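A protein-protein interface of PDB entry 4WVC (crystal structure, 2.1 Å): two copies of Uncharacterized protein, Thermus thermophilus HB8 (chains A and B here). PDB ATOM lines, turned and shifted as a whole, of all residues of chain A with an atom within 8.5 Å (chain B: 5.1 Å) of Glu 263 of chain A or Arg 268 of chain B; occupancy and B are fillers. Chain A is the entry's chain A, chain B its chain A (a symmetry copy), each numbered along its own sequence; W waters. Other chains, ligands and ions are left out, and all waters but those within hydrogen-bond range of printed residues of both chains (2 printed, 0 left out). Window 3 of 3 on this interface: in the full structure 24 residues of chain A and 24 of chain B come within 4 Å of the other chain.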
ATOM      1  N   LEU A 136      22.944  32.195  30.015  1.00  0.00           N
ATOM      2  CA  LEU A 136      22.909  30.830  29.514  1.00  0.00           C
ATOM      3  C   LEU A 136      21.713  30.034  30.056  1.00  0.00           C
ATOM      4  O   LEU A 136      21.079  29.276  29.324  1.00  0.00           O
ATOM      5  CB  LEU A 136      24.230  30.155  29.902  1.00  0.00           C
ATOM      6  CG  LEU A 136      24.601  28.861  29.214  1.00  0.00           C
ATOM      7  CD1 LEU A 136      24.742  29.084  27.714  1.00  0.00           C
ATOM      8  CD2 LEU A 136      25.892  28.342  29.822  1.00  0.00           C
ATOM      9  N   GLN A 242      18.153  34.708  17.975  1.00  0.00           N
ATOM     10  CA  GLN A 242      19.288  34.323  17.118  1.00  0.00           C
ATOM     11  C   GLN A 242      20.413  35.364  17.287  1.00  0.00           C
ATOM     12  O   GLN A 242      21.601  35.021  17.371  1.00  0.00           O
ATOM     13  CB  GLN A 242      18.857  34.172  15.650  1.00  0.00           C
ATOM     14  CG  GLN A 242      19.988  34.027  14.603  1.00  0.00           C
ATOM     15  CD  GLN A 242      20.739  32.676  14.594  1.00  0.00           C
ATOM     16  OE1 GLN A 242      21.772  32.511  13.925  1.00  0.00           O
ATOM     17  NE2 GLN A 242      20.208  31.713  15.322  1.00  0.00           N
ATOM     18  N   ASN A 245      21.940  34.922  20.746  1.00  0.00           N
ATOM     19  CA  ASN A 245      22.788  33.718  20.748  1.00  0.00           C
ATOM     20  C   ASN A 245      24.168  34.012  20.158  1.00  0.00           C
ATOM     21  O   ASN A 245      25.186  33.656  20.753  1.00  0.00           O
ATOM     22  CB  ASN A 245      22.101  32.548  20.002  1.00  0.00           C
ATOM     23  CG  ASN A 245      21.076  31.814  20.864  1.00  0.00           C
ATOM     24  OD1 ASN A 245      21.161  31.770  22.105  1.00  0.00           O
ATOM     25  ND2 ASN A 245      20.121  31.199  20.211  1.00  0.00           N
ATOM     26  N   ARG A 246      24.197  34.691  19.018  1.00  0.00           N
ATOM     27  CA  ARG A 246      25.456  35.044  18.386  1.00  0.00           C
ATOM     28  C   ARG A 246      26.297  35.960  19.286  1.00  0.00           C
ATOM     29  O   ARG A 246      27.521  35.810  19.363  1.00  0.00           O
ATOM     30  CB  ARG A 246      25.207  35.669  17.013  1.00  0.00           C
ATOM     31  CG  ARG A 246      24.600  34.673  16.033  1.00  0.00           C
ATOM     32  CD  ARG A 246      24.646  35.129  14.597  1.00  0.00           C
ATOM     33  NE  ARG A 246      24.238  34.064  13.654  1.00  0.00           N
ATOM     34  CZ  ARG A 246      25.048  33.158  13.085  1.00  0.00           C
ATOM     35  NH1 ARG A 246      26.346  33.132  13.331  1.00  0.00           N
ATOM     36  NH2 ARG A 246      24.541  32.259  12.241  1.00  0.00           N
ATOM     37  N   LEU A 248      25.973  36.099  22.686  1.00  0.00           N
ATOM     38  CA  LEU A 248      26.361  35.266  23.834  1.00  0.00           C
ATOM     39  C   LEU A 248      27.585  34.403  23.504  1.00  0.00           C
ATOM     40  O   LEU A 248      28.478  34.277  24.326  1.00  0.00           O
ATOM     41  CB  LEU A 248      25.199  34.384  24.278  1.00  0.00           C
ATOM     42  CG  LEU A 248      25.353  33.683  25.621  1.00  0.00           C
ATOM     43  CD1 LEU A 248      25.658  34.669  26.743  1.00  0.00           C
ATOM     44  CD2 LEU A 248      24.084  32.886  25.916  1.00  0.00           C
ATOM     45  N   TYR A 249      27.634  33.854  22.281  1.00  0.00           N
ATOM     46  CA  TYR A 249      28.814  33.137  21.782  1.00  0.00           C
ATOM     47  C   TYR A 249      30.084  34.020  21.827  1.00  0.00           C
ATOM     48  O   TYR A 249      31.149  33.561  22.261  1.00  0.00           O
ATOM     49  CB  TYR A 249      28.602  32.654  20.346  1.00  0.00           C
ATOM     50  CG  TYR A 249      29.865  32.118  19.713  1.00  0.00           C
ATOM     51  CD1 TYR A 249      30.734  32.957  19.041  1.00  0.00           C
ATOM     52  CD2 TYR A 249      30.204  30.767  19.807  1.00  0.00           C
ATOM     53  CE1 TYR A 249      31.915  32.495  18.486  1.00  0.00           C
ATOM     54  CE2 TYR A 249      31.374  30.288  19.236  1.00  0.00           C
ATOM     55  CZ  TYR A 249      32.229  31.163  18.577  1.00  0.00           C
ATOM     56  OH  TYR A 249      33.389  30.712  17.983  1.00  0.00           O
ATOM     57  N   ALA A 252      31.309  34.507  25.366  1.00  0.00           N
ATOM     58  CA  ALA A 252      31.945  33.296  25.828  1.00  0.00           C
ATOM     59  C   ALA A 252      33.391  33.236  25.376  1.00  0.00           C
ATOM     60  O   ALA A 252      34.267  32.930  26.162  1.00  0.00           O
ATOM     61  CB  ALA A 252      31.183  32.067  25.346  1.00  0.00           C
ATOM     62  N   VAL A 253      33.640  33.459  24.093  1.00  0.00           N
ATOM     63  CA  VAL A 253      34.979  33.357  23.555  1.00  0.00           C
ATOM     64  C   VAL A 253      35.847  34.458  24.185  1.00  0.00           C
ATOM     65  O   VAL A 253      36.977  34.199  24.592  1.00  0.00           O
ATOM     66  CB  VAL A 253      34.990  33.475  22.018  1.00  0.00           C
ATOM     67  CG1 VAL A 253      36.409  33.451  21.509  1.00  0.00           C
ATOM     68  CG2 VAL A 253      34.192  32.340  21.375  1.00  0.00           C
ATOM     69  N   GLU A 257      34.968  31.433  28.484  1.00  0.00           N
ATOM     70  CA  GLU A 257      33.989  30.509  29.085  1.00  0.00           C
ATOM     71  C   GLU A 257      33.661  29.442  28.080  1.00  0.00           C
ATOM     72  O   GLU A 257      33.759  29.652  26.861  1.00  0.00           O
ATOM     73  CB  GLU A 257      32.692  31.220  29.438  1.00  0.00           C
ATOM     74  CG  GLU A 257      32.866  32.421  30.346  1.00  0.00           C
ATOM     75  CD  GLU A 257      32.926  32.058  31.805  1.00  0.00           C
ATOM     76  OE1 GLU A 257      32.838  30.862  32.104  1.00  0.00           O
ATOM     77  OE2 GLU A 257      33.069  32.950  32.661  1.00  0.00           O
ATOM     78  N   ASP A 258      33.322  28.280  28.605  1.00  0.00           N
ATOM     79  CA  ASP A 258      32.865  27.171  27.819  1.00  0.00           C
ATOM     80  C   ASP A 258      31.576  27.602  27.156  1.00  0.00           C
ATOM     81  O   ASP A 258      30.605  27.873  27.851  1.00  0.00           O
ATOM     82  CB  ASP A 258      32.626  25.966  28.742  1.00  0.00           C
ATOM     83  CG  ASP A 258      32.551  24.660  27.992  1.00  0.00           C
ATOM     84  OD1 ASP A 258      32.155  24.665  26.808  1.00  0.00           O
ATOM     85  OD2 ASP A 258      32.898  23.619  28.590  1.00  0.00           O
ATOM     86  N   PRO A 259      31.551  27.664  25.807  1.00  0.00           N
ATOM     87  CA  PRO A 259      30.315  28.050  25.146  1.00  0.00           C
ATOM     88  C   PRO A 259      29.246  26.965  25.168  1.00  0.00           C
ATOM     89  O   PRO A 259      28.135  27.223  24.738  1.00  0.00           O
ATOM     90  CB  PRO A 259      30.762  28.334  23.728  1.00  0.00           C
ATOM     91  CG  PRO A 259      31.940  27.413  23.506  1.00  0.00           C
ATOM     92  CD  PRO A 259      32.601  27.276  24.842  1.00  0.00           C
ATOM     93  N   TYR A 260      29.558  25.779  25.680  1.00  0.00           N
ATOM     94  CA  TYR A 260      28.601  24.677  25.775  1.00  0.00           C
ATOM     95  C   TYR A 260      27.808  24.540  24.465  1.00  0.00           C
ATOM     96  O   TYR A 260      28.423  24.418  23.398  1.00  0.00           O
ATOM     97  CB  TYR A 260      27.705  24.817  27.014  1.00  0.00           C
ATOM     98  CG  TYR A 260      28.421  24.468  28.296  1.00  0.00           C
ATOM     99  CD1 TYR A 260      28.798  23.158  28.552  1.00  0.00           C
ATOM    100  CD2 TYR A 260      28.745  25.440  29.223  1.00  0.00           C
ATOM    101  CE1 TYR A 260      29.461  22.820  29.701  1.00  0.00           C
ATOM    102  CE2 TYR A 260      29.415  25.118  30.398  1.00  0.00           C
ATOM    103  CZ  TYR A 260      29.782  23.807  30.622  1.00  0.00           C
ATOM    104  OH  TYR A 260      30.443  23.473  31.770  1.00  0.00           O
ATOM    105  N   GLU A 261      26.476  24.570  24.524  1.00  0.00           N
ATOM    106  CA  GLU A 261      25.647  24.278  23.351  1.00  0.00           C
ATOM    107  C   GLU A 261      25.208  25.534  22.588  1.00  0.00           C
ATOM    108  O   GLU A 261      24.269  25.484  21.816  1.00  0.00           O
ATOM    109  CB  GLU A 261      24.420  23.427  23.743  1.00  0.00           C
ATOM    110  CG  GLU A 261      23.261  24.149  24.462  1.00  0.00           C
ATOM    111  CD  GLU A 261      23.415  24.218  25.979  1.00  0.00           C
ATOM    112  OE1 GLU A 261      22.408  24.046  26.724  1.00  0.00           O
ATOM    113  OE2 GLU A 261      24.555  24.428  26.445  1.00  0.00           O
ATOM    114  N   ILE A 262      25.883  26.663  22.796  1.00  0.00           N
ATOM    115  CA  ILE A 262      25.472  27.902  22.141  1.00  0.00           C
ATOM    116  C   ILE A 262      25.589  27.774  20.622  1.00  0.00           C
ATOM    117  O   ILE A 262      24.680  28.190  19.906  1.00  0.00           O
ATOM    118  CB  ILE A 262      26.254  29.126  22.660  1.00  0.00           C
ATOM    119  CG1 ILE A 262      25.836  29.435  24.111  1.00  0.00           C
ATOM    120  CG2 ILE A 262      25.985  30.349  21.787  1.00  0.00           C
ATOM    121  CD1 ILE A 262      26.806  30.337  24.838  1.00  0.00           C
ATOM    122  N   GLU A 263      26.688  27.189  20.149  1.00  0.00           N
ATOM    123  CA  GLU A 263      26.905  26.956  18.716  1.00  0.00           C
ATOM    124  C   GLU A 263      25.744  26.213  18.085  1.00  0.00           C
ATOM    125  O   GLU A 263      25.269  26.568  17.012  1.00  0.00           O
ATOM    126  CB  GLU A 263      28.161  26.120  18.492  1.00  0.00           C
ATOM    127  CG  GLU A 263      29.454  26.856  18.784  1.00  0.00           C
ATOM    128  CD  GLU A 263      30.109  26.461  20.112  1.00  0.00           C
ATOM    129  OE1 GLU A 263      29.429  26.434  21.184  1.00  0.00           O
ATOM    130  OE2 GLU A 263      31.323  26.200  20.070  1.00  0.00           O
ATOM    131  N   GLU A 264      25.307  25.177  18.788  1.00  0.00           N
ATOM    132  CA  GLU A 264      24.147  24.377  18.439  1.00  0.00           C
ATOM    133  C   GLU A 264      22.877  25.235  18.324  1.00  0.00           C
ATOM    134  O   GLU A 264      22.131  25.138  17.351  1.00  0.00           O
ATOM    135  CB  GLU A 264      23.995  23.312  19.513  1.00  0.00           C
ATOM    136  CG  GLU A 264      22.843  22.354  19.381  1.00  0.00           C
ATOM    137  CD  GLU A 264      23.097  21.112  20.227  1.00  0.00           C
ATOM    138  OE1 GLU A 264      23.440  20.058  19.654  1.00  0.00           O
ATOM    139  OE2 GLU A 264      23.021  21.192  21.467  1.00  0.00           O
ATOM    140  N   TRP A 265      22.650  26.094  19.305  1.00  0.00           N
ATOM    141  CA  TRP A 265      21.532  27.007  19.225  1.00  0.00           C
ATOM    142  C   TRP A 265      21.624  27.876  17.959  1.00  0.00           C
ATOM    143  O   TRP A 265      20.631  28.084  17.283  1.00  0.00           O
ATOM    144  CB  TRP A 265      21.467  27.901  20.456  1.00  0.00           C
ATOM    145  CG  TRP A 265      21.163  27.216  21.714  1.00  0.00           C
ATOM    146  CD1 TRP A 265      20.496  26.040  21.883  1.00  0.00           C
ATOM    147  CD2 TRP A 265      21.463  27.701  23.030  1.00  0.00           C
ATOM    148  NE1 TRP A 265      20.385  25.746  23.229  1.00  0.00           N
ATOM    149  CE2 TRP A 265      20.961  26.759  23.951  1.00  0.00           C
ATOM    150  CE3 TRP A 265      22.102  28.852  23.519  1.00  0.00           C
ATOM    151  CZ2 TRP A 265      21.078  26.925  25.329  1.00  0.00           C
ATOM    152  CZ3 TRP A 265      22.232  29.019  24.897  1.00  0.00           C
ATOM    153  CH2 TRP A 265      21.720  28.057  25.785  1.00  0.00           C
ATOM    154  N   ILE A 266      22.809  28.390  17.671  1.00  0.00           N
ATOM    155  CA  ILE A 266      23.020  29.291  16.558  1.00  0.00           C
ATOM    156  C   ILE A 266      22.773  28.617  15.195  1.00  0.00           C
ATOM    157  O   ILE A 266      22.074  29.158  14.345  1.00  0.00           O
ATOM    158  CB  ILE A 266      24.453  29.876  16.607  1.00  0.00           C
ATOM    159  CG1 ILE A 266      24.570  30.834  17.792  1.00  0.00           C
ATOM    160  CG2 ILE A 266      24.782  30.578  15.293  1.00  0.00           C
ATOM    161  CD1 ILE A 266      25.953  31.381  18.034  1.00  0.00           C
ATOM    162  N   VAL A 267      23.351  27.433  15.022  1.00  0.00           N
ATOM    163  CA  VAL A 267      23.274  26.679  13.778  1.00  0.00           C
ATOM    164  C   VAL A 267      21.854  26.202  13.495  1.00  0.00           C
ATOM    165  O   VAL A 267      21.332  26.415  12.422  1.00  0.00           O
ATOM    166  CB  VAL A 267      24.304  25.500  13.786  1.00  0.00           C
ATOM    167  CG1 VAL A 267      24.061  24.543  12.636  1.00  0.00           C
ATOM    168  CG2 VAL A 267      25.730  26.050  13.736  1.00  0.00           C
ATOM    169  N   ARG A 268      21.222  25.594  14.483  1.00  0.00           N
ATOM    170  CA  ARG A 268      19.838  25.176  14.391  1.00  0.00           C
ATOM    171  C   ARG A 268      18.882  26.387  14.288  1.00  0.00           C
ATOM    172  O   ARG A 268      17.894  26.346  13.541  1.00  0.00           O
ATOM    173  CB  ARG A 268      19.520  24.299  15.595  1.00  0.00           C
ATOM    174  CG  ARG A 268      18.266  23.484  15.487  1.00  0.00           C
ATOM    175  CD  ARG A 268      18.141  22.592  16.701  1.00  0.00           C
ATOM    176  NE  ARG A 268      19.272  21.665  16.748  1.00  0.00           N
ATOM    177  CZ  ARG A 268      19.863  21.209  17.845  1.00  0.00           C
ATOM    178  NH1 ARG A 268      19.467  21.583  19.060  1.00  0.00           N
ATOM    179  NH2 ARG A 268      20.884  20.356  17.729  1.00  0.00           N
ATOM    180  N   GLY A 269      19.196  27.481  14.982  1.00  0.00           N
ATOM    181  CA  GLY A 269      18.370  28.682  14.922  1.00  0.00           C
ATOM    182  C   GLY A 269      18.378  29.341  13.558  1.00  0.00           C
ATOM    183  O   GLY A 269      17.371  29.929  13.116  1.00  0.00           O
ATOM    184  N   GLU A 270      19.502  29.219  12.864  1.00  0.00           N
ATOM    185  CA  GLU A 270      19.644  29.832  11.564  1.00  0.00           C
ATOM    186  C   GLU A 270      18.815  29.093  10.508  1.00  0.00           C
ATOM    187  O   GLU A 270      18.180  29.719   9.686  1.00  0.00           O
ATOM    188  CB  GLU A 270      21.102  29.900  11.173  1.00  0.00           C
ATOM    189  CG  GLU A 270      21.341  30.669   9.903  1.00  0.00           C
ATOM    190  CD  GLU A 270      22.805  30.782   9.561  1.00  0.00           C
ATOM    191  OE1 GLU A 270      23.613  29.927   9.976  1.00  0.00           O
ATOM    192  OE2 GLU A 270      23.155  31.720   8.848  1.00  0.00           O
ATOM    193  N   ARG B 150      36.521  24.449  22.540  1.00  0.00           N
ATOM    194  CA  ARG B 150      35.764  24.029  21.380  1.00  0.00           C
ATOM    195  C   ARG B 150      34.869  25.169  20.863  1.00  0.00           C
ATOM    196  O   ARG B 150      33.682  24.971  20.606  1.00  0.00           O
ATOM    197  CB  ARG B 150      34.980  22.744  21.683  1.00  0.00           C
ATOM    198  CG  ARG B 150      35.872  21.633  22.254  1.00  0.00           C
ATOM    199  CD  ARG B 150      35.157  20.311  22.592  1.00  0.00           C
ATOM    200  NE  ARG B 150      33.734  20.263  22.195  1.00  0.00           N
ATOM    201  CZ  ARG B 150      33.241  19.693  21.079  1.00  0.00           C
ATOM    202  NH1 ARG B 150      34.037  19.091  20.191  1.00  0.00           N
ATOM    203  NH2 ARG B 150      31.935  19.728  20.835  1.00  0.00           N
ATOM    204  N   THR B 151      35.496  26.342  20.679  1.00  0.00           N
ATOM    205  CA  THR B 151      34.866  27.558  20.140  1.00  0.00           C
ATOM    206  C   THR B 151      34.705  27.564  18.611  1.00  0.00           C
ATOM    207  O   THR B 151      33.861  28.285  18.064  1.00  0.00           O
ATOM    208  CB  THR B 151      35.686  28.813  20.502  1.00  0.00           C
ATOM    209  OG1 THR B 151      37.008  28.750  19.933  1.00  0.00           O
ATOM    210  CG2 THR B 151      35.794  28.959  22.025  1.00  0.00           C
ATOM    211  N   GLY B 152      35.560  26.806  17.932  1.00  0.00           N
ATOM    212  CA  GLY B 152      35.679  26.883  16.492  1.00  0.00           C
ATOM    213  C   GLY B 152      36.786  27.810  16.042  1.00  0.00           C
ATOM    214  O   GLY B 152      37.131  27.811  14.873  1.00  0.00           O
ATOM    215  N   GLU B 263      33.422  18.599   8.806  1.00  0.00           N
ATOM    216  CA  GLU B 263      32.158  19.342   8.731  1.00  0.00           C
ATOM    217  C   GLU B 263      31.921  20.175   9.975  1.00  0.00           C
ATOM    218  O   GLU B 263      31.541  21.338   9.900  1.00  0.00           O
ATOM    219  CB  GLU B 263      30.979  18.385   8.589  1.00  0.00           C
ATOM    220  CG  GLU B 263      30.900  17.698   7.238  1.00  0.00           C
ATOM    221  CD  GLU B 263      31.359  16.236   7.255  1.00  0.00           C
ATOM    222  OE1 GLU B 263      32.465  15.914   7.790  1.00  0.00           O
ATOM    223  OE2 GLU B 263      30.605  15.418   6.706  1.00  0.00           O
ATOM    224  N   GLU B 264      32.163  19.541  11.115  1.00  0.00           N
ATOM    225  CA  GLU B 264      32.104  20.159  12.428  1.00  0.00           C
ATOM    226  C   GLU B 264      33.053  21.364  12.533  1.00  0.00           C
ATOM    227  O   GLU B 264      32.665  22.439  12.986  1.00  0.00           O
ATOM    228  CB  GLU B 264      32.461  19.088  13.446  1.00  0.00           C
ATOM    229  CG  GLU B 264      32.482  19.490  14.895  1.00  0.00           C
ATOM    230  CD  GLU B 264      32.389  18.253  15.781  1.00  0.00           C
ATOM    231  OE1 GLU B 264      31.304  18.001  16.343  1.00  0.00           O
ATOM    232  OE2 GLU B 264      33.369  17.491  15.872  1.00  0.00           O
ATOM    233  N   TRP B 265      34.287  21.189  12.086  1.00  0.00           N
ATOM    234  CA  TRP B 265      35.212  22.298  12.057  1.00  0.00           C
ATOM    235  C   TRP B 265      34.652  23.456  11.214  1.00  0.00           C
ATOM    236  O   TRP B 265      34.748  24.606  11.606  1.00  0.00           O
ATOM    237  CB  TRP B 265      36.565  21.870  11.505  1.00  0.00           C
ATOM    238  CG  TRP B 265      37.310  20.922  12.336  1.00  0.00           C
ATOM    239  CD1 TRP B 265      37.208  20.733  13.682  1.00  0.00           C
ATOM    240  CD2 TRP B 265      38.351  20.044  11.884  1.00  0.00           C
ATOM    241  NE1 TRP B 265      38.107  19.768  14.095  1.00  0.00           N
ATOM    242  CE2 TRP B 265      38.826  19.341  13.009  1.00  0.00           C
ATOM    243  CE3 TRP B 265      38.934  19.793  10.632  1.00  0.00           C
ATOM    244  CZ2 TRP B 265      39.853  18.403  12.925  1.00  0.00           C
ATOM    245  CZ3 TRP B 265      39.954  18.848  10.539  1.00  0.00           C
ATOM    246  CH2 TRP B 265      40.402  18.165  11.684  1.00  0.00           C
ATOM    247  N   ILE B 266      34.098  23.138  10.054  1.00  0.00           N
ATOM    248  CA  ILE B 266      33.606  24.133   9.125  1.00  0.00           C
ATOM    249  C   ILE B 266      32.416  24.932   9.687  1.00  0.00           C
ATOM    250  O   ILE B 266      32.397  26.157   9.623  1.00  0.00           O
ATOM    251  CB  ILE B 266      33.209  23.464   7.785  1.00  0.00           C
ATOM    252  CG1 ILE B 266      34.468  22.981   7.067  1.00  0.00           C
ATOM    253  CG2 ILE B 266      32.418  24.441   6.921  1.00  0.00           C
ATOM    254  CD1 ILE B 266      34.219  22.195   5.805  1.00  0.00           C
ATOM    255  N   VAL B 267      31.445  24.213  10.240  1.00  0.00           N
ATOM    256  CA  VAL B 267      30.220  24.795  10.770  1.00  0.00           C
ATOM    257  C   VAL B 267      30.490  25.659  11.996  1.00  0.00           C
ATOM    258  O   VAL B 267      30.066  26.792  12.061  1.00  0.00           O
ATOM    259  CB  VAL B 267      29.160  23.678  11.054  1.00  0.00           C
ATOM    260  CG1 VAL B 267      27.989  24.215  11.853  1.00  0.00           C
ATOM    261  CG2 VAL B 267      28.677  23.066   9.739  1.00  0.00           C
ATOM    262  N   ARG B 268      31.238  25.126  12.947  1.00  0.00           N
ATOM    263  CA  ARG B 268      31.658  25.862  14.121  1.00  0.00           C
ATOM    264  C   ARG B 268      32.627  27.011  13.757  1.00  0.00           C
ATOM    265  O   ARG B 268      32.551  28.104  14.336  1.00  0.00           O
ATOM    266  CB  ARG B 268      32.280  24.881  15.106  1.00  0.00           C
ATOM    267  CG  ARG B 268      32.438  25.387  16.508  1.00  0.00           C
ATOM    268  CD  ARG B 268      32.965  24.275  17.387  1.00  0.00           C
ATOM    269  NE  ARG B 268      32.002  23.174  17.416  1.00  0.00           N
ATOM    270  CZ  ARG B 268      32.296  21.882  17.501  1.00  0.00           C
ATOM    271  NH1 ARG B 268      33.554  21.453  17.557  1.00  0.00           N
ATOM    272  NH2 ARG B 268      31.303  20.988  17.525  1.00  0.00           N
ATOM    273  N   GLY B 269      33.494  26.796  12.768  1.00  0.00           N
ATOM    274  CA  GLY B 269      34.425  27.832  12.335  1.00  0.00           C
ATOM    275  C   GLY B 269      33.737  29.022  11.699  1.00  0.00           C
ATOM    276  O   GLY B 269      34.189  30.177  11.824  1.00  0.00           O
ATOM    277  N   GLU B 270      32.616  28.756  11.039  1.00  0.00           N
ATOM    278  CA  GLU B 270      31.886  29.802  10.362  1.00  0.00           C
ATOM    279  C   GLU B 270      31.177  30.722  11.361  1.00  0.00           C
ATOM    280  O   GLU B 270      31.187  31.923  11.194  1.00  0.00           O
ATOM    281  CB  GLU B 270      30.911  29.205   9.373  1.00  0.00           C
ATOM    282  CG  GLU B 270      30.230  30.234   8.515  1.00  0.00           C
ATOM    283  CD  GLU B 270      29.309  29.619   7.493  1.00  0.00           C
ATOM    284  OE1 GLU B 270      28.809  28.494   7.696  1.00  0.00           O
ATOM    285  OE2 GLU B 270      29.058  30.272   6.482  1.00  0.00           O
ATOM    286  N   VAL B 271      30.612  30.149  12.411  1.00  0.00           N
ATOM    287  CA  VAL B 271      30.050  30.929  13.486  1.00  0.00           C
ATOM    288  C   VAL B 271      31.164  31.784  14.083  1.00  0.00           C
ATOM    289  O   VAL B 271      30.987  32.994  14.324  1.00  0.00           O
ATOM    290  CB  VAL B 271      29.443  30.037  14.606  1.00  0.00           C
ATOM    291  CG1 VAL B 271      29.099  30.879  15.821  1.00  0.00           C
ATOM    292  CG2 VAL B 271      28.242  29.247  14.104  1.00  0.00           C
ATOM    293  N   GLY B 272      32.309  31.166  14.344  1.00  0.00           N
ATOM    294  CA  GLY B 272      33.428  31.884  14.977  1.00  0.00           C
ATOM    295  C   GLY B 272      33.995  33.037  14.148  1.00  0.00           C
ATOM    296  O   GLY B 272      34.221  34.153  14.665  1.00  0.00           O
HETATM  297  O   HOH W   1      28.047  32.302  10.978  1.00  0.00           O
HETATM  298  O   HOH W   2      28.706  34.495  14.865  1.00  0.00           O
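Of the 22 printed residues of chain A, 5 touch a printed residue of chain B.
Hydrophobic or aromatic side chains of chain A within 4 Å of the printed part of chain B: Tyr 249, Val 253, Ile 266 and Val 267.
Of the 13 printed residues of chain B, 6 touch a printed residue of chain A.
Printed residues of chain B that touch a printed residue of chain A: Arg 150, Thr 151, Val 267, Arg 268, Val 271 and Gly 272.
Hydrophobic or aromatic side chains of chain B within 4 Å of the printed part of chain A: Val 267 and Val 271.
Water W2 bridges O of Val 271 of chain B (2.8 Å) and NH1 of Arg 246 of chain A (3.1 Å).
Water W1 bridges NH1 of Arg 246 of chain A and O of Glu 270 of chain B.
OH of Tyr 249 of chain A sits at hydrogen-bond distance from O of Thr 151 of chain B (2.5 Å).
The side-chain carboxylate (OE2) of Glu 263 of chain A sits close to the backbone carbonyl oxygen (O) of Arg 150 of chain B, at 2.7 Å.
Among the printed residues, merely in contact across the chains: Tyr 249 of chain A with Gly 272 of chain B, Val 267 of chain A with Val 267 of chain B, Glu 263 of chain A with Arg 268 of chain B, Glu 263 of chain A with Thr 151 of chain B, Val 253 of chain A with Thr 151 of chain B and Ile 266 of chain A with Val 271 of chain B.
The side-chain amide nitrogen (NE2) of Gln 242 of chain A lies within hydrogen-bond range of the backbone carbonyl oxygen (O) of Ile 266 of chain A, at 3.3 Å.
OE1 of Glu 264 of chain B is in salt-bridge range of NH2 of Arg 268 of chain B (3.2 Å).
Printed residues of chain B within 4 Å of Tyr 249 of chain A: Thr 151 and Gly 272.
Of the printed residues of chain B, Glu 263 of chain A touches Arg 150, Thr 151 and Arg 268.
Glu 264 of chain A touches none of the printed residues of chain B.
Of the printed residues of chain B, Val 267 of chain A touches Val 267 (3.5 Å).
Of the printed residues of chain A, Arg 150 of chain B touches Glu 263.
Glu 264 of chain B touches none of the printed residues of chain A.
Printed residues of chain A within 4 Å of Arg 268 of chain B: Glu 263 (3.7 Å).
Of the printed residues of chain A, Val 271 of chain B touches Ile 266.
Glu 263 of chain A touches Arg 268 of chain B, but with the chains exchanged Arg 268 of chain A does not touch Glu 263 of chain B (12.1 Å).
Val 267 of chain B touches its own counterpart, Val 267 of chain A.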
